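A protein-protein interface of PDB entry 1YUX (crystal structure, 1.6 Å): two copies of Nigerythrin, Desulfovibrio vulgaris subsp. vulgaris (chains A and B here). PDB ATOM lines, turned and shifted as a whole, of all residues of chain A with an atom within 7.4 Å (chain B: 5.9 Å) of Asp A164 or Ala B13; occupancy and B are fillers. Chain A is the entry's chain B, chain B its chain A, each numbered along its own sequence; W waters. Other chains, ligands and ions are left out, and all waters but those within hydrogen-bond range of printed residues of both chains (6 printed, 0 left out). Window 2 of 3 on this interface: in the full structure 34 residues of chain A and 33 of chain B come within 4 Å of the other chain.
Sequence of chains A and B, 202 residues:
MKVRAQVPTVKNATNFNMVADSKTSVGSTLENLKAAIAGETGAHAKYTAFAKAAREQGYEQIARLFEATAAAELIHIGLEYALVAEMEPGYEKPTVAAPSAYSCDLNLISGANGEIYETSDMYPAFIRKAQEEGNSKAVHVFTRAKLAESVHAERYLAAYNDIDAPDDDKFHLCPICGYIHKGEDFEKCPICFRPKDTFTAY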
ATOM      1  N   TYR A  59     -24.872  33.932  30.506  1.00  0.00           N
ATOM      2  CA  TYR A  59     -24.043  32.757  30.252  1.00  0.00           C
ATOM      3  C   TYR A  59     -23.135  32.544  31.452  1.00  0.00           C
ATOM      4  O   TYR A  59     -21.938  32.838  31.404  1.00  0.00           O
ATOM      5  CB  TYR A  59     -23.188  32.956  29.001  1.00  0.00           C
ATOM      6  CG  TYR A  59     -23.969  33.200  27.731  1.00  0.00           C
ATOM      7  CD1 TYR A  59     -24.111  34.487  27.213  1.00  0.00           C
ATOM      8  CD2 TYR A  59     -24.511  32.138  27.014  1.00  0.00           C
ATOM      9  CE1 TYR A  59     -24.765  34.705  26.000  1.00  0.00           C
ATOM     10  CE2 TYR A  59     -25.170  32.346  25.801  1.00  0.00           C
ATOM     11  CZ  TYR A  59     -25.286  33.631  25.299  1.00  0.00           C
ATOM     12  OH  TYR A  59     -25.883  33.837  24.076  1.00  0.00           O
ATOM     13  N   ILE A  62     -20.142  30.012  30.818  1.00  0.00           N
ATOM     14  CA  ILE A  62     -19.110  30.592  29.968  1.00  0.00           C
ATOM     15  C   ILE A  62     -18.339  31.651  30.749  1.00  0.00           C
ATOM     16  O   ILE A  62     -17.126  31.784  30.593  1.00  0.00           O
ATOM     17  CB  ILE A  62     -19.716  31.198  28.680  1.00  0.00           C
ATOM     18  CG1 ILE A  62     -20.198  30.061  27.771  1.00  0.00           C
ATOM     19  CG2 ILE A  62     -18.676  32.059  27.956  1.00  0.00           C
ATOM     20  CD1 ILE A  62     -20.960  30.522  26.537  1.00  0.00           C
ATOM     21  N   ALA A 159     -17.226  25.708  24.093  1.00  0.00           N
ATOM     22  CA  ALA A 159     -18.243  26.550  24.709  1.00  0.00           C
ATOM     23  C   ALA A 159     -19.064  27.237  23.630  1.00  0.00           C
ATOM     24  O   ALA A 159     -20.273  27.419  23.775  1.00  0.00           O
ATOM     25  CB  ALA A 159     -17.590  27.582  25.609  1.00  0.00           C
ATOM     26  N   TYR A 160     -18.398  27.620  22.546  1.00  0.00           N
ATOM     27  CA  TYR A 160     -19.058  28.286  21.429  1.00  0.00           C
ATOM     28  C   TYR A 160     -20.054  27.332  20.774  1.00  0.00           C
ATOM     29  O   TYR A 160     -21.193  27.697  20.496  1.00  0.00           O
ATOM     30  CB  TYR A 160     -18.005  28.720  20.410  1.00  0.00           C
ATOM     31  CG  TYR A 160     -18.541  29.436  19.191  1.00  0.00           C
ATOM     32  CD1 TYR A 160     -18.699  30.821  19.184  1.00  0.00           C
ATOM     33  CD2 TYR A 160     -18.828  28.733  18.024  1.00  0.00           C
ATOM     34  CE1 TYR A 160     -19.122  31.491  18.033  1.00  0.00           C
ATOM     35  CE2 TYR A 160     -19.252  29.389  16.873  1.00  0.00           C
ATOM     36  CZ  TYR A 160     -19.392  30.766  16.883  1.00  0.00           C
ATOM     37  OH  TYR A 160     -19.773  31.417  15.734  1.00  0.00           O
ATOM     38  N   ASN A 161     -19.622  26.100  20.542  1.00  0.00           N
ATOM     39  CA  ASN A 161     -20.483  25.109  19.911  1.00  0.00           C
ATOM     40  C   ASN A 161     -21.706  24.772  20.746  1.00  0.00           C
ATOM     41  O   ASN A 161     -22.771  24.496  20.200  1.00  0.00           O
ATOM     42  CB  ASN A 161     -19.687  23.842  19.601  1.00  0.00           C
ATOM     43  CG  ASN A 161     -18.752  24.038  18.443  1.00  0.00           C
ATOM     44  OD1 ASN A 161     -19.040  24.831  17.556  1.00  0.00           O
ATOM     45  ND2 ASN A 161     -17.637  23.320  18.432  1.00  0.00           N
ATOM     46  N   ASP A 162     -21.549  24.797  22.066  1.00  0.00           N
ATOM     47  CA  ASP A 162     -22.653  24.505  22.975  1.00  0.00           C
ATOM     48  C   ASP A 162     -23.084  25.765  23.714  1.00  0.00           C
ATOM     49  O   ASP A 162     -23.502  25.701  24.869  1.00  0.00           O
ATOM     50  CB  ASP A 162     -22.243  23.449  24.007  1.00  0.00           C
ATOM     51  CG  ASP A 162     -22.095  22.070  23.408  1.00  0.00           C
ATOM     52  OD1 ASP A 162     -22.894  21.728  22.511  1.00  0.00           O
ATOM     53  OD2 ASP A 162     -21.190  21.326  23.847  1.00  0.00           O
ATOM     54  N   ILE A 163     -22.993  26.909  23.046  1.00  0.00           N
ATOM     55  CA  ILE A 163     -23.353  28.173  23.677  1.00  0.00           C
ATOM     56  C   ILE A 163     -24.776  28.183  24.238  1.00  0.00           C
ATOM     57  O   ILE A 163     -25.043  28.838  25.244  1.00  0.00           O
ATOM     58  CB  ILE A 163     -23.157  29.357  22.690  1.00  0.00           C
ATOM     59  CG1 ILE A 163     -23.261  30.686  23.443  1.00  0.00           C
ATOM     60  CG2 ILE A 163     -24.186  29.292  21.570  1.00  0.00           C
ATOM     61  CD1 ILE A 163     -22.795  31.883  22.634  1.00  0.00           C
ATOM     62  N   ASP A 164     -25.684  27.447  23.607  1.00  0.00           N
ATOM     63  CA  ASP A 164     -27.062  27.402  24.082  1.00  0.00           C
ATOM     64  C   ASP A 164     -27.392  26.083  24.771  1.00  0.00           C
ATOM     65  O   ASP A 164     -28.561  25.737  24.962  1.00  0.00           O
ATOM     66  CB  ASP A 164     -28.017  27.648  22.917  1.00  0.00           C
ATOM     67  CG  ASP A 164     -27.741  28.966  22.220  1.00  0.00           C
ATOM     68  OD1 ASP A 164     -27.722  30.005  22.914  1.00  0.00           O
ATOM     69  OD2 ASP A 164     -27.543  28.962  20.988  1.00  0.00           O
ATOM     70  N   ALA A 165     -26.350  25.354  25.154  1.00  0.00           N
ATOM     71  CA  ALA A 165     -26.514  24.077  25.836  1.00  0.00           C
ATOM     72  C   ALA A 165     -25.493  23.967  26.959  1.00  0.00           C
ATOM     73  O   ALA A 165     -24.673  23.047  26.986  1.00  0.00           O
ATOM     74  CB  ALA A 165     -26.339  22.927  24.852  1.00  0.00           C
ATOM     75  N   PRO A 166     -25.518  24.919  27.898  1.00  0.00           N
ATOM     76  CA  PRO A 166     -24.568  24.871  29.008  1.00  0.00           C
ATOM     77  C   PRO A 166     -24.992  23.781  29.982  1.00  0.00           C
ATOM     78  O   PRO A 166     -26.095  23.245  29.886  1.00  0.00           O
ATOM     79  CB  PRO A 166     -24.696  26.259  29.616  1.00  0.00           C
ATOM     80  CG  PRO A 166     -26.168  26.535  29.451  1.00  0.00           C
ATOM     81  CD  PRO A 166     -26.411  26.085  28.020  1.00  0.00           C
ATOM     82  N   ARG B   4     -29.576  19.488  21.241  1.00  0.00           N
ATOM     83  CA  ARG B   4     -30.581  20.297  21.922  1.00  0.00           C
ATOM     84  C   ARG B   4     -31.964  19.714  21.653  1.00  0.00           C
ATOM     85  O   ARG B   4     -32.121  18.842  20.798  1.00  0.00           O
ATOM     86  CB  ARG B   4     -30.533  21.743  21.418  1.00  0.00           C
ATOM     87  CG  ARG B   4     -29.275  22.515  21.788  1.00  0.00           C
ATOM     88  CD  ARG B   4     -29.218  23.845  21.035  1.00  0.00           C
ATOM     89  NE  ARG B   4     -30.380  24.684  21.313  1.00  0.00           N
ATOM     90  CZ  ARG B   4     -30.721  25.753  20.599  1.00  0.00           C
ATOM     91  NH1 ARG B   4     -29.989  26.122  19.555  1.00  0.00           N
ATOM     92  NH2 ARG B   4     -31.799  26.456  20.926  1.00  0.00           N
ATOM     93  N   PRO B   8     -30.746  23.434  15.915  1.00  0.00           N
ATOM     94  CA  PRO B   8     -30.165  24.780  15.940  1.00  0.00           C
ATOM     95  C   PRO B   8     -30.424  25.579  14.666  1.00  0.00           C
ATOM     96  O   PRO B   8     -30.239  25.078  13.556  1.00  0.00           O
ATOM     97  CB  PRO B   8     -28.673  24.517  16.149  1.00  0.00           C
ATOM     98  CG  PRO B   8     -28.636  23.186  16.825  1.00  0.00           C
ATOM     99  CD  PRO B   8     -29.703  22.411  16.099  1.00  0.00           C
ATOM    100  N   THR B   9     -30.850  26.825  14.836  1.00  0.00           N
ATOM    101  CA  THR B   9     -31.125  27.705  13.706  1.00  0.00           C
ATOM    102  C   THR B   9     -30.728  29.123  14.086  1.00  0.00           C
ATOM    103  O   THR B   9     -30.480  29.414  15.255  1.00  0.00           O
ATOM    104  CB  THR B   9     -32.620  27.726  13.345  1.00  0.00           C
ATOM    105  OG1 THR B   9     -33.354  28.338  14.410  1.00  0.00           O
ATOM    106  CG2 THR B   9     -33.139  26.315  13.120  1.00  0.00           C
ATOM    107  N   VAL B  10     -30.676  30.008  13.100  1.00  0.00           N
ATOM    108  CA  VAL B  10     -30.319  31.391  13.369  1.00  0.00           C
ATOM    109  C   VAL B  10     -31.374  32.019  14.279  1.00  0.00           C
ATOM    110  O   VAL B  10     -31.112  33.013  14.952  1.00  0.00           O
ATOM    111  CB  VAL B  10     -30.218  32.207  12.058  1.00  0.00           C
ATOM    112  CG1 VAL B  10     -31.582  32.280  11.380  1.00  0.00           C
ATOM    113  CG2 VAL B  10     -29.685  33.599  12.352  1.00  0.00           C
ATOM    114  N   LYS B  11     -32.560  31.420  14.309  1.00  0.00           N
ATOM    115  CA  LYS B  11     -33.662  31.930  15.125  1.00  0.00           C
ATOM    116  C   LYS B  11     -33.613  31.524  16.597  1.00  0.00           C
ATOM    117  O   LYS B  11     -34.055  32.280  17.465  1.00  0.00           O
ATOM    118  CB  LYS B  11     -35.000  31.483  14.524  1.00  0.00           C
ATOM    119  CG  LYS B  11     -36.229  32.018  15.243  1.00  0.00           C
ATOM    120  CD  LYS B  11     -37.505  31.467  14.618  1.00  0.00           C
ATOM    121  CE  LYS B  11     -38.753  32.045  15.273  1.00  0.00           C
ATOM    122  NZ  LYS B  11     -38.876  33.515  15.044  1.00  0.00           N
ATOM    123  N   ASN B  12     -33.085  30.339  16.892  1.00  0.00           N
ATOM    124  CA  ASN B  12     -33.036  29.885  18.279  1.00  0.00           C
ATOM    125  C   ASN B  12     -31.637  29.760  18.874  1.00  0.00           C
ATOM    126  O   ASN B  12     -31.493  29.333  20.019  1.00  0.00           O
ATOM    127  CB  ASN B  12     -33.757  28.540  18.435  1.00  0.00           C
ATOM    128  CG  ASN B  12     -33.065  27.406  17.696  1.00  0.00           C
ATOM    129  OD1 ASN B  12     -31.844  27.410  17.521  1.00  0.00           O
ATOM    130  ND2 ASN B  12     -33.844  26.415  17.275  1.00  0.00           N
ATOM    131  N   ALA B  13     -30.616  30.126  18.105  1.00  0.00           N
ATOM    132  CA  ALA B  13     -29.237  30.031  18.581  1.00  0.00           C
ATOM    133  C   ALA B  13     -28.623  31.402  18.835  1.00  0.00           C
ATOM    134  O   ALA B  13     -29.082  32.409  18.301  1.00  0.00           O
ATOM    135  CB  ALA B  13     -28.394  29.259  17.575  1.00  0.00           C
ATOM    136  N   THR B  14     -27.573  31.443  19.648  1.00  0.00           N
ATOM    137  CA  THR B  14     -26.942  32.717  19.953  1.00  0.00           C
ATOM    138  C   THR B  14     -25.485  32.823  19.520  1.00  0.00           C
ATOM    139  O   THR B  14     -24.753  33.681  20.008  1.00  0.00           O
ATOM    140  CB  THR B  14     -27.052  33.040  21.458  1.00  0.00           C
ATOM    141  OG1 THR B  14     -26.407  32.017  22.223  1.00  0.00           O
ATOM    142  CG2 THR B  14     -28.518  33.127  21.873  1.00  0.00           C
ATOM    143  N   ASN B  15     -25.056  31.948  18.618  1.00  0.00           N
ATOM    144  CA  ASN B  15     -23.689  32.028  18.123  1.00  0.00           C
ATOM    145  C   ASN B  15     -23.678  32.302  16.623  1.00  0.00           C
ATOM    146  O   ASN B  15     -22.848  31.775  15.885  1.00  0.00           O
ATOM    147  CB  ASN B  15     -22.886  30.758  18.468  1.00  0.00           C
ATOM    148  CG  ASN B  15     -23.520  29.480  17.941  1.00  0.00           C
ATOM    149  OD1 ASN B  15     -24.626  29.486  17.405  1.00  0.00           O
ATOM    150  ND2 ASN B  15     -22.810  28.367  18.102  1.00  0.00           N
ATOM    151  N   PHE B  16     -24.607  33.148  16.181  1.00  0.00           N
ATOM    152  CA  PHE B  16     -24.703  33.514  14.775  1.00  0.00           C
ATOM    153  C   PHE B  16     -24.309  34.959  14.494  1.00  0.00           C
ATOM    154  O   PHE B  16     -24.562  35.471  13.407  1.00  0.00           O
ATOM    155  CB  PHE B  16     -26.112  33.257  14.235  1.00  0.00           C
ATOM    156  CG  PHE B  16     -26.370  31.822  13.884  1.00  0.00           C
ATOM    157  CD1 PHE B  16     -26.489  30.860  14.879  1.00  0.00           C
ATOM    158  CD2 PHE B  16     -26.471  31.428  12.553  1.00  0.00           C
ATOM    159  CE1 PHE B  16     -26.704  29.524  14.557  1.00  0.00           C
ATOM    160  CE2 PHE B  16     -26.687  30.092  12.220  1.00  0.00           C
ATOM    161  CZ  PHE B  16     -26.803  29.141  13.229  1.00  0.00           C
ATOM    162  N   LEU B 147     -22.888  25.848  11.168  1.00  0.00           N
ATOM    163  CA  LEU B 147     -22.870  25.040  12.380  1.00  0.00           C
ATOM    164  C   LEU B 147     -21.815  23.944  12.337  1.00  0.00           C
ATOM    165  O   LEU B 147     -21.189  23.639  13.349  1.00  0.00           O
ATOM    166  CB  LEU B 147     -24.251  24.425  12.622  1.00  0.00           C
ATOM    167  CG  LEU B 147     -25.346  25.443  12.940  1.00  0.00           C
ATOM    168  CD1 LEU B 147     -26.703  24.774  12.832  1.00  0.00           C
ATOM    169  CD2 LEU B 147     -25.131  26.023  14.335  1.00  0.00           C
HETATM  170  O   HOH W   1     -20.243  34.012  16.115  1.00  0.00           O
HETATM  171  O   HOH W   2     -27.230  26.661  19.636  1.00  0.00           O
HETATM  172  O   HOH W   3     -23.413  25.525  17.649  1.00  0.00           O
HETATM  173  O   HOH W   4     -21.934  23.995  15.908  1.00  0.00           O
HETATM  174  O   HOH W   5     -31.740  24.826  23.906  1.00  0.00           O
HETATM  175  O   HOH W   6     -23.977  35.359  22.172  1.00  0.00           O
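No position is printed for both chains.
Hydrophobic or aromatic side chains of chain B that line the printed part of chain A: Ala B13.
Printed residues of chain A that touch a printed residue of chain B: Tyr A59, Tyr A160, Ile A163 and Asp A164.
Hydrophobic or aromatic side chains of chain A that line the printed part of chain B: Tyr A59, Tyr A160 and Ile A163.
Among the printed residues, no Asp or Glu carboxylate lies within 4 Å of a Lys or Arg side-chain nitrogen of the other chain.
Water W1 lies within hydrogen-bond range of OH of Tyr A160 (2.7 Å) and O of Asn B15 (3.4 Å).
Water W2 bridges the side-chain carboxylate of Asp A164 (2.7 Å) and the guanidinium group of Arg B4 (2.8 Å).
Water W4 bridges O of Leu B147 (2.7 Å) and OD1 of Asn A161 (3.4 Å).
Water W3 lies within hydrogen-bond range of O of Asn A161 and ND2 of Asn B15.
Water W6 lies within hydrogen-bond range of the backbone carbonyl oxygen of Thr B14 (2.8 Å) and the side-chain hydroxyl of Tyr A59 (3.1 Å).
Water W5 bridges NE of Arg B4 (2.9 Å) and O of Asp A164 (3.5 Å).
Of the printed residues of chain B, Tyr A59 touches Thr B14 (2.6 Å).
Printed residues of chain B within 4 Å of Tyr A160: Asn B15 (3.0 Å).
Of the printed residues of chain B, Ile A163 touches Thr B14 (3.6 Å) and Asn B15 (3.7 Å).
Of the printed residues of chain B, Asp A164 touches Ala B13 and Thr B14.
Ala B13 touches just one residue of chain A: Asp A164.
Of the printed residues of chain A, Thr B14 touches Tyr A59, Ile A163 and Asp A164.
Of the printed residues of chain A, Asn B15 touches Tyr A160 and Ile A163.
Phe B16 touches none of the printed residues of chain A.
The nearest printed residue of chain A that does not touch Asn B15 is Asn A161 (4.4 Å).
Among the printed residues, pairs that only touch across the chains: Asp A164 with Ala B13 (3.1 Å), Ile A163 with Thr B14 (3.6 Å) and Ile A163 with Asn B15 (3.7 Å).
OH of Tyr A59 sits at hydrogen-bond distance from OG1 of Thr B14 (2.6 Å).
The side-chain hydroxyl of Thr B14 sits at hydrogen-bond distance from the side-chain carboxylate of Asp A164, 2.5 Å away.
The side-chain amide nitrogen (ND2) of Asn B15 lies within hydrogen-bond range of the backbone carbonyl oxygen (O) of Tyr A160 (3.0 Å).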
